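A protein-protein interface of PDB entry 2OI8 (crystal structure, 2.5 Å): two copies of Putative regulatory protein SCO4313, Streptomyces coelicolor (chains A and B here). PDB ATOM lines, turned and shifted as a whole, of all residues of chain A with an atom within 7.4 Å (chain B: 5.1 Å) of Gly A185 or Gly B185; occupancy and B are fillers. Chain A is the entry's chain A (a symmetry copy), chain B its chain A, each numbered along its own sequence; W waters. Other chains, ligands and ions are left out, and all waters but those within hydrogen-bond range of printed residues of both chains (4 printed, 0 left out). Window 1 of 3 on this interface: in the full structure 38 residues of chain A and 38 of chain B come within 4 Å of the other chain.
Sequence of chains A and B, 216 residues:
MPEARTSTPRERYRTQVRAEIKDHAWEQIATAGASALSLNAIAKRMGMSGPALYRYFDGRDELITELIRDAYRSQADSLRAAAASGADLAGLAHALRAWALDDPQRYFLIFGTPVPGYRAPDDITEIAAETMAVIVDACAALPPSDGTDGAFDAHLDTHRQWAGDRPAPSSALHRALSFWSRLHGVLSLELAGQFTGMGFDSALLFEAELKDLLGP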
ATOM      1  N   TYR A 107      39.640  11.728  31.949  1.00  0.00           N
ATOM      2  CA  TYR A 107      38.360  11.340  31.372  1.00  0.00           C
ATOM      3  C   TYR A 107      38.470   9.938  30.765  1.00  0.00           C
ATOM      4  O   TYR A 107      37.611   9.068  30.996  1.00  0.00           O
ATOM      5  CB  TYR A 107      37.920  12.376  30.307  1.00  0.00           C
ATOM      6  CG  TYR A 107      36.609  12.038  29.587  1.00  0.00           C
ATOM      7  CD1 TYR A 107      36.623  11.282  28.415  1.00  0.00           C
ATOM      8  CD2 TYR A 107      35.359  12.491  30.079  1.00  0.00           C
ATOM      9  CE1 TYR A 107      35.423  10.950  27.731  1.00  0.00           C
ATOM     10  CE2 TYR A 107      34.138  12.177  29.397  1.00  0.00           C
ATOM     11  CZ  TYR A 107      34.191  11.400  28.239  1.00  0.00           C
ATOM     12  OH  TYR A 107      33.037  11.062  27.543  1.00  0.00           O
ATOM     13  N   PHE A 179      20.904  11.805  29.834  1.00  0.00           N
ATOM     14  CA  PHE A 179      21.808  12.918  30.077  1.00  0.00           C
ATOM     15  C   PHE A 179      23.253  12.384  30.052  1.00  0.00           C
ATOM     16  O   PHE A 179      24.121  12.900  29.354  1.00  0.00           O
ATOM     17  CB  PHE A 179      21.408  13.536  31.428  1.00  0.00           C
ATOM     18  CG  PHE A 179      22.349  14.577  31.968  1.00  0.00           C
ATOM     19  CD1 PHE A 179      23.504  14.209  32.645  1.00  0.00           C
ATOM     20  CD2 PHE A 179      22.032  15.931  31.873  1.00  0.00           C
ATOM     21  CE1 PHE A 179      24.353  15.160  33.165  1.00  0.00           C
ATOM     22  CE2 PHE A 179      22.876  16.896  32.404  1.00  0.00           C
ATOM     23  CZ  PHE A 179      24.034  16.510  33.053  1.00  0.00           C
ATOM     24  N   TRP A 180      23.488  11.331  30.821  1.00  0.00           N
ATOM     25  CA  TRP A 180      24.794  10.706  30.915  1.00  0.00           C
ATOM     26  C   TRP A 180      25.326  10.325  29.522  1.00  0.00           C
ATOM     27  O   TRP A 180      26.431  10.704  29.137  1.00  0.00           O
ATOM     28  CB  TRP A 180      24.668   9.465  31.792  1.00  0.00           C
ATOM     29  CG  TRP A 180      25.927   8.951  32.374  1.00  0.00           C
ATOM     30  CD1 TRP A 180      26.414   7.684  32.270  1.00  0.00           C
ATOM     31  CD2 TRP A 180      26.854   9.674  33.174  1.00  0.00           C
ATOM     32  NE1 TRP A 180      27.593   7.572  32.949  1.00  0.00           N
ATOM     33  CE2 TRP A 180      27.893   8.781  33.513  1.00  0.00           C
ATOM     34  CE3 TRP A 180      26.916  10.993  33.638  1.00  0.00           C
ATOM     35  CZ2 TRP A 180      28.987   9.158  34.313  1.00  0.00           C
ATOM     36  CZ3 TRP A 180      28.022  11.376  34.436  1.00  0.00           C
ATOM     37  CH2 TRP A 180      29.036  10.455  34.757  1.00  0.00           C
ATOM     38  N   SER A 181      24.525   9.600  28.753  1.00  0.00           N
ATOM     39  CA  SER A 181      25.040   9.019  27.531  1.00  0.00           C
ATOM     40  C   SER A 181      25.116  10.063  26.450  1.00  0.00           C
ATOM     41  O   SER A 181      26.104  10.126  25.751  1.00  0.00           O
ATOM     42  CB  SER A 181      24.182   7.849  27.094  1.00  0.00           C
ATOM     43  OG  SER A 181      22.908   8.344  26.764  1.00  0.00           O
ATOM     44  N   ARG A 182      24.090  10.890  26.315  1.00  0.00           N
ATOM     45  CA  ARG A 182      24.104  11.962  25.317  1.00  0.00           C
ATOM     46  C   ARG A 182      25.304  12.938  25.424  1.00  0.00           C
ATOM     47  O   ARG A 182      25.942  13.260  24.407  1.00  0.00           O
ATOM     48  CB  ARG A 182      22.775  12.732  25.314  1.00  0.00           C
ATOM     49  CG  ARG A 182      21.655  11.926  24.721  1.00  0.00           C
ATOM     50  CD  ARG A 182      20.357  12.692  24.577  1.00  0.00           C
ATOM     51  NE  ARG A 182      19.238  11.766  24.352  1.00  0.00           N
ATOM     52  CZ  ARG A 182      17.951  12.121  24.289  1.00  0.00           C
ATOM     53  NH1 ARG A 182      17.589  13.386  24.427  1.00  0.00           N
ATOM     54  NH2 ARG A 182      17.019  11.201  24.090  1.00  0.00           N
ATOM     55  N   LEU A 183      25.608  13.390  26.639  1.00  0.00           N
ATOM     56  CA  LEU A 183      26.711  14.345  26.872  1.00  0.00           C
ATOM     57  C   LEU A 183      28.126  13.742  26.804  1.00  0.00           C
ATOM     58  O   LEU A 183      29.107  14.428  26.440  1.00  0.00           O
ATOM     59  CB  LEU A 183      26.491  15.066  28.211  1.00  0.00           C
ATOM     60  CG  LEU A 183      25.170  15.846  28.252  1.00  0.00           C
ATOM     61  CD1 LEU A 183      25.033  16.528  29.576  1.00  0.00           C
ATOM     62  CD2 LEU A 183      25.043  16.854  27.114  1.00  0.00           C
ATOM     63  N   HIS A 184      28.229  12.467  27.186  1.00  0.00           N
ATOM     64  CA  HIS A 184      29.466  11.708  27.003  1.00  0.00           C
ATOM     65  C   HIS A 184      29.735  11.431  25.535  1.00  0.00           C
ATOM     66  O   HIS A 184      30.893  11.425  25.114  1.00  0.00           O
ATOM     67  CB  HIS A 184      29.455  10.434  27.822  1.00  0.00           C
ATOM     68  CG  HIS A 184      29.738  10.674  29.271  1.00  0.00           C
ATOM     69  ND1 HIS A 184      30.998  10.988  29.736  1.00  0.00           N
ATOM     70  CD2 HIS A 184      28.922  10.678  30.353  1.00  0.00           C
ATOM     71  CE1 HIS A 184      30.947  11.176  31.045  1.00  0.00           C
ATOM     72  NE2 HIS A 184      29.700  10.981  31.446  1.00  0.00           N
ATOM     73  N   GLY A 185      28.654  11.242  24.767  1.00  0.00           N
ATOM     74  CA  GLY A 185      28.719  11.038  23.322  1.00  0.00           C
ATOM     75  C   GLY A 185      29.448  12.203  22.713  1.00  0.00           C
ATOM     76  O   GLY A 185      30.396  12.011  21.971  1.00  0.00           O
ATOM     77  N   VAL A 186      29.046  13.424  23.057  1.00  0.00           N
ATOM     78  CA  VAL A 186      29.763  14.572  22.502  1.00  0.00           C
ATOM     79  C   VAL A 186      31.122  14.844  23.166  1.00  0.00           C
ATOM     80  O   VAL A 186      32.083  15.116  22.477  1.00  0.00           O
ATOM     81  CB  VAL A 186      28.879  15.823  22.303  1.00  0.00           C
ATOM     82  CG1 VAL A 186      27.481  15.593  22.800  1.00  0.00           C
ATOM     83  CG2 VAL A 186      29.520  17.086  22.883  1.00  0.00           C
ATOM     84  N   LEU A 187      31.224  14.685  24.475  1.00  0.00           N
ATOM     85  CA  LEU A 187      32.504  14.897  25.129  1.00  0.00           C
ATOM     86  C   LEU A 187      33.591  13.967  24.630  1.00  0.00           C
ATOM     87  O   LEU A 187      34.708  14.406  24.333  1.00  0.00           O
ATOM     88  CB  LEU A 187      32.374  14.805  26.661  1.00  0.00           C
ATOM     89  CG  LEU A 187      31.617  15.973  27.290  1.00  0.00           C
ATOM     90  CD1 LEU A 187      31.439  15.736  28.782  1.00  0.00           C
ATOM     91  CD2 LEU A 187      32.324  17.306  26.998  1.00  0.00           C
ATOM     92  N   SER A 188      33.290  12.687  24.521  1.00  0.00           N
ATOM     93  CA  SER A 188      34.353  11.786  24.123  1.00  0.00           C
ATOM     94  C   SER A 188      34.594  11.822  22.629  1.00  0.00           C
ATOM     95  O   SER A 188      35.711  11.609  22.177  1.00  0.00           O
ATOM     96  CB  SER A 188      34.092  10.387  24.630  1.00  0.00           C
ATOM     97  OG  SER A 188      32.778  10.040  24.327  1.00  0.00           O
ATOM     98  N   LEU A 189      33.574  12.152  21.848  1.00  0.00           N
ATOM     99  CA  LEU A 189      33.810  12.370  20.417  1.00  0.00           C
ATOM    100  C   LEU A 189      34.689  13.550  20.197  1.00  0.00           C
ATOM    101  O   LEU A 189      35.563  13.484  19.360  1.00  0.00           O
ATOM    102  CB  LEU A 189      32.524  12.522  19.601  1.00  0.00           C
ATOM    103  CG  LEU A 189      31.745  11.232  19.330  1.00  0.00           C
ATOM    104  CD1 LEU A 189      30.499  11.592  18.553  1.00  0.00           C
ATOM    105  CD2 LEU A 189      32.587  10.216  18.546  1.00  0.00           C
ATOM    106  N   GLU A 190      34.489  14.634  20.945  1.00  0.00           N
ATOM    107  CA  GLU A 190      35.403  15.773  20.792  1.00  0.00           C
ATOM    108  C   GLU A 190      36.800  15.499  21.325  1.00  0.00           C
ATOM    109  O   GLU A 190      37.776  15.707  20.598  1.00  0.00           O
ATOM    110  CB  GLU A 190      34.831  17.121  21.259  1.00  0.00           C
ATOM    111  CG  GLU A 190      34.321  17.245  22.663  1.00  0.00           C
ATOM    112  CD  GLU A 190      33.336  18.430  22.809  1.00  0.00           C
ATOM    113  OE1 GLU A 190      33.540  19.490  22.157  1.00  0.00           O
ATOM    114  OE2 GLU A 190      32.351  18.307  23.581  1.00  0.00           O
ATOM    115  N   LEU A 191      36.887  14.971  22.549  1.00  0.00           N
ATOM    116  CA  LEU A 191      38.167  14.523  23.145  1.00  0.00           C
ATOM    117  C   LEU A 191      38.901  13.411  22.362  1.00  0.00           C
ATOM    118  O   LEU A 191      40.126  13.298  22.439  1.00  0.00           O
ATOM    119  CB  LEU A 191      37.939  14.072  24.592  1.00  0.00           C
ATOM    120  CG  LEU A 191      37.583  15.186  25.597  1.00  0.00           C
ATOM    121  CD1 LEU A 191      37.461  14.634  27.038  1.00  0.00           C
ATOM    122  CD2 LEU A 191      38.657  16.269  25.562  1.00  0.00           C
ATOM    123  N   PHE A 195      35.829  15.594  15.730  1.00  0.00           N
ATOM    124  CA  PHE A 195      35.228  16.789  15.137  1.00  0.00           C
ATOM    125  C   PHE A 195      36.323  17.738  14.621  1.00  0.00           C
ATOM    126  O   PHE A 195      36.045  18.852  14.181  1.00  0.00           O
ATOM    127  CB  PHE A 195      34.329  17.514  16.154  1.00  0.00           C
ATOM    128  CG  PHE A 195      33.169  16.682  16.688  1.00  0.00           C
ATOM    129  CD1 PHE A 195      32.361  15.930  15.834  1.00  0.00           C
ATOM    130  CD2 PHE A 195      32.869  16.693  18.048  1.00  0.00           C
ATOM    131  CE1 PHE A 195      31.276  15.171  16.330  1.00  0.00           C
ATOM    132  CE2 PHE A 195      31.781  15.948  18.559  1.00  0.00           C
ATOM    133  CZ  PHE A 195      30.983  15.190  17.685  1.00  0.00           C
ATOM    134  N   LEU A 205      27.071  22.256  19.487  1.00  0.00           N
ATOM    135  CA  LEU A 205      26.495  20.899  19.485  1.00  0.00           C
ATOM    136  C   LEU A 205      26.143  20.421  20.903  1.00  0.00           C
ATOM    137  O   LEU A 205      25.023  19.964  21.149  1.00  0.00           O
ATOM    138  CB  LEU A 205      27.400  19.884  18.774  1.00  0.00           C
ATOM    139  CG  LEU A 205      26.951  18.427  18.967  1.00  0.00           C
ATOM    140  CD1 LEU A 205      25.532  18.144  18.453  1.00  0.00           C
ATOM    141  CD2 LEU A 205      27.948  17.435  18.380  1.00  0.00           C
ATOM    142  N   TRP B 180      24.880  10.513  15.567  1.00  0.00           N
ATOM    143  CA  TRP B 180      26.264  10.130  15.772  1.00  0.00           C
ATOM    144  C   TRP B 180      26.633  10.173  17.266  1.00  0.00           C
ATOM    145  O   TRP B 180      27.125   9.195  17.829  1.00  0.00           O
ATOM    146  CB  TRP B 180      27.147  11.087  14.980  1.00  0.00           C
ATOM    147  CG  TRP B 180      28.519  10.615  14.691  1.00  0.00           C
ATOM    148  CD1 TRP B 180      29.681  11.265  14.978  1.00  0.00           C
ATOM    149  CD2 TRP B 180      28.885   9.408  14.035  1.00  0.00           C
ATOM    150  NE1 TRP B 180      30.750  10.534  14.551  1.00  0.00           N
ATOM    151  CE2 TRP B 180      30.294   9.383  13.969  1.00  0.00           C
ATOM    152  CE3 TRP B 180      28.162   8.335  13.497  1.00  0.00           C
ATOM    153  CZ2 TRP B 180      31.008   8.329  13.369  1.00  0.00           C
ATOM    154  CZ3 TRP B 180      28.880   7.269  12.903  1.00  0.00           C
ATOM    155  CH2 TRP B 180      30.286   7.284  12.851  1.00  0.00           C
ATOM    156  N   SER B 181      26.367  11.298  17.916  1.00  0.00           N
ATOM    157  CA  SER B 181      26.888  11.490  19.254  1.00  0.00           C
ATOM    158  C   SER B 181      26.056  10.729  20.251  1.00  0.00           C
ATOM    159  O   SER B 181      26.606  10.090  21.121  1.00  0.00           O
ATOM    160  CB  SER B 181      26.933  12.964  19.601  1.00  0.00           C
ATOM    161  OG  SER B 181      25.611  13.442  19.641  1.00  0.00           O
ATOM    162  N   ARG B 182      24.738  10.780  20.125  1.00  0.00           N
ATOM    163  CA  ARG B 182      23.858  10.033  21.027  1.00  0.00           C
ATOM    164  C   ARG B 182      24.126   8.507  21.083  1.00  0.00           C
ATOM    165  O   ARG B 182      24.190   7.921  22.178  1.00  0.00           O
ATOM    166  CB  ARG B 182      22.381  10.315  20.716  1.00  0.00           C
ATOM    167  CG  ARG B 182      21.968  11.695  21.139  1.00  0.00           C
ATOM    168  CD  ARG B 182      20.487  11.971  20.974  1.00  0.00           C
ATOM    169  NE  ARG B 182      20.224  13.414  21.046  1.00  0.00           N
ATOM    170  CZ  ARG B 182      19.035  13.987  20.833  1.00  0.00           C
ATOM    171  NH1 ARG B 182      17.973  13.255  20.536  1.00  0.00           N
ATOM    172  NH2 ARG B 182      18.910  15.302  20.914  1.00  0.00           N
ATOM    173  N   LEU B 183      24.291   7.879  19.919  1.00  0.00           N
ATOM    174  CA  LEU B 183      24.526   6.423  19.836  1.00  0.00           C
ATOM    175  C   LEU B 183      25.945   5.965  20.219  1.00  0.00           C
ATOM    176  O   LEU B 183      26.150   4.835  20.715  1.00  0.00           O
ATOM    177  CB  LEU B 183      24.155   5.924  18.430  1.00  0.00           C
ATOM    178  CG  LEU B 183      22.685   6.189  18.079  1.00  0.00           C
ATOM    179  CD1 LEU B 183      22.395   5.667  16.708  1.00  0.00           C
ATOM    180  CD2 LEU B 183      21.716   5.591  19.096  1.00  0.00           C
ATOM    181  N   HIS B 184      26.924   6.834  19.958  1.00  0.00           N
ATOM    182  CA  HIS B 184      28.290   6.618  20.431  1.00  0.00           C
ATOM    183  C   HIS B 184      28.385   6.759  21.939  1.00  0.00           C
ATOM    184  O   HIS B 184      29.157   6.041  22.575  1.00  0.00           O
ATOM    185  CB  HIS B 184      29.269   7.529  19.719  1.00  0.00           C
ATOM    186  CG  HIS B 184      29.600   7.059  18.339  1.00  0.00           C
ATOM    187  ND1 HIS B 184      30.412   5.969  18.104  1.00  0.00           N
ATOM    188  CD2 HIS B 184      29.207   7.508  17.122  1.00  0.00           C
ATOM    189  CE1 HIS B 184      30.505   5.765  16.799  1.00  0.00           C
ATOM    190  NE2 HIS B 184      29.794   6.693  16.181  1.00  0.00           N
ATOM    191  N   GLY B 185      27.564   7.660  22.495  1.00  0.00           N
ATOM    192  CA  GLY B 185      27.466   7.877  23.936  1.00  0.00           C
ATOM    193  C   GLY B 185      27.127   6.566  24.588  1.00  0.00           C
ATOM    194  O   GLY B 185      27.805   6.148  25.512  1.00  0.00           O
ATOM    195  N   VAL B 186      26.105   5.877  24.086  1.00  0.00           N
ATOM    196  CA  VAL B 186      25.778   4.583  24.685  1.00  0.00           C
ATOM    197  C   VAL B 186      26.728   3.446  24.278  1.00  0.00           C
ATOM    198  O   VAL B 186      27.125   2.666  25.119  1.00  0.00           O
ATOM    199  CB  VAL B 186      24.276   4.226  24.619  1.00  0.00           C
ATOM    200  CG1 VAL B 186      23.495   5.273  23.879  1.00  0.00           C
ATOM    201  CG2 VAL B 186      24.039   2.811  24.083  1.00  0.00           C
ATOM    202  N   LEU B 187      27.160   3.405  23.029  1.00  0.00           N
ATOM    203  CA  LEU B 187      28.088   2.366  22.620  1.00  0.00           C
ATOM    204  C   LEU B 187      29.396   2.399  23.386  1.00  0.00           C
ATOM    205  O   LEU B 187      29.874   1.362  23.860  1.00  0.00           O
ATOM    206  CB  LEU B 187      28.348   2.409  21.103  1.00  0.00           C
ATOM    207  CG  LEU B 187      27.155   1.973  20.256  1.00  0.00           C
ATOM    208  CD1 LEU B 187      27.466   2.159  18.780  1.00  0.00           C
ATOM    209  CD2 LEU B 187      26.751   0.526  20.582  1.00  0.00           C
ATOM    210  N   SER B 188      29.986   3.571  23.527  1.00  0.00           N
ATOM    211  CA  SER B 188      31.276   3.591  24.186  1.00  0.00           C
ATOM    212  C   SER B 188      31.141   3.514  25.692  1.00  0.00           C
ATOM    213  O   SER B 188      32.013   2.982  26.366  1.00  0.00           O
ATOM    214  CB  SER B 188      32.090   4.782  23.741  1.00  0.00           C
ATOM    215  OG  SER B 188      31.292   5.920  23.809  1.00  0.00           O
ATOM    216  N   LEU B 189      30.026   3.985  26.235  1.00  0.00           N
ATOM    217  CA  LEU B 189      29.781   3.769  27.666  1.00  0.00           C
ATOM    218  C   LEU B 189      29.617   2.321  27.966  1.00  0.00           C
ATOM    219  O   LEU B 189      30.140   1.864  28.958  1.00  0.00           O
ATOM    220  CB  LEU B 189      28.579   4.550  28.204  1.00  0.00           C
ATOM    221  CG  LEU B 189      28.794   6.051  28.412  1.00  0.00           C
ATOM    222  CD1 LEU B 189      27.493   6.645  28.907  1.00  0.00           C
ATOM    223  CD2 LEU B 189      29.921   6.329  29.416  1.00  0.00           C
ATOM    224  N   GLU B 190      28.911   1.577  27.116  1.00  0.00           N
ATOM    225  CA  GLU B 190      28.812   0.133  27.361  1.00  0.00           C
ATOM    226  C   GLU B 190      30.120  -0.607  27.128  1.00  0.00           C
ATOM    227  O   GLU B 190      30.562  -1.346  28.013  1.00  0.00           O
ATOM    228  CB  GLU B 190      27.606  -0.549  26.696  1.00  0.00           C
ATOM    229  CG  GLU B 190      27.422  -0.413  25.214  1.00  0.00           C
ATOM    230  CD  GLU B 190      25.956  -0.680  24.796  1.00  0.00           C
ATOM    231  OE1 GLU B 190      25.290  -1.567  25.396  1.00  0.00           O
ATOM    232  OE2 GLU B 190      25.461  -0.001  23.858  1.00  0.00           O
HETATM  233  O   HOH W   1      17.876  10.238  21.326  1.00  0.00           O
HETATM  234  O   HOH W   2      19.631  15.674  23.853  1.00  0.00           O
HETATM  235  O   HOH W   3      24.599  13.316  22.181  1.00  0.00           O
HETATM  236  O   HOH W   4      22.737   8.914  24.092  1.00  0.00           O
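Leu B189 touches Trp A180.
Ser A181 touches Gly B185.
CD1 of Leu B189 touches CA of Ser A181, at 3.7 Å.
Arg A182 touches Arg B182 (CG to CG, 3.6 Å).
Gly A185 touches Ser B181 (CA to O, 3.2 Å).
Gly A185 touches Gly B185.
CD1 of Trp B180 touches CD1 of Leu A189, at 3.7 Å.
CA of Ser B181 touches CD1 of Leu A189, 3.7 Å away.
Gly A185 touches just these residues of chain B: Ser B181 (3.2 Å) and Gly B185 (3.5 Å).
Of chain A, only Ser A181 and Gly A185 come within 4 Å of Gly B185.
Of the printed residues of chain B, Ser A181 touches Gly B185 and Leu B189.
Printed residues of chain A within 4 Å of Leu B189: Trp A180 (3.7 Å) and Ser A181 (3.7 Å).
Glu B190 touches none of the printed residues of chain A.
The nearest residue of chain B that does not touch Gly A185 is His B184 (4.5 Å).
The nearest printed residue of chain A that does not touch Ser B181 is Val A186 (4.1 Å).
Of the 11 printed residues of chain B, 5 touch a printed residue of chain A.
Along chain B the printed residues that touch a printed residue of chain A span positions 180 to 189.
Printed residues of chain A that touch a printed residue of chain B: Trp A180, Ser A181, Arg A182, Gly A185 and Leu A189.
Among the printed residues, 8 pairs touch across the chains.
Among the printed residues, no Asp or Glu carboxylate lies within 4 Å of a Lys or Arg side-chain nitrogen of the other chain.
Ser A181 touches Gly B185, and with the chains exchanged Gly A185 touches Ser B181.
Ser A181 touches Leu B189, and with the chains exchanged Leu A189 touches Ser B181.
Arg B182 touches its own counterpart, Arg A182.
Gly A185 touches its own counterpart, Gly B185.
Positions printed for both chains: 180, 181, 182, 183, 184, 185, 186, 187, 188, 189 and 190.
Of the 8 pairs that touch across the chains among the printed residues, 8 have their exchanged pair printed and touching as well.
Water W4 lies within hydrogen-bond range of the backbone carbonyl oxygen (O) of Arg B182 (2.6 Å), the side-chain hydroxyl (OG) of Ser A181 (2.7 Å) and the backbone NH (N) of Arg A182 (3.3 Å).
Water W3 lies within hydrogen-bond range of the backbone carbonyl oxygen of Arg A182 (2.6 Å), the side-chain hydroxyl of Ser B181 (2.7 Å) and the backbone NH of Arg B182 (3.3 Å).
Water W1 lies within hydrogen-bond range of the guanidinium group (NH2) of Arg A182 (3.0 Å) and the guanidinium group (NH1) of Arg B182 (3.1 Å).
Water W2 bridges NH2 of Arg B182 (3.0 Å) and NH1 of Arg A182 (3.1 Å).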
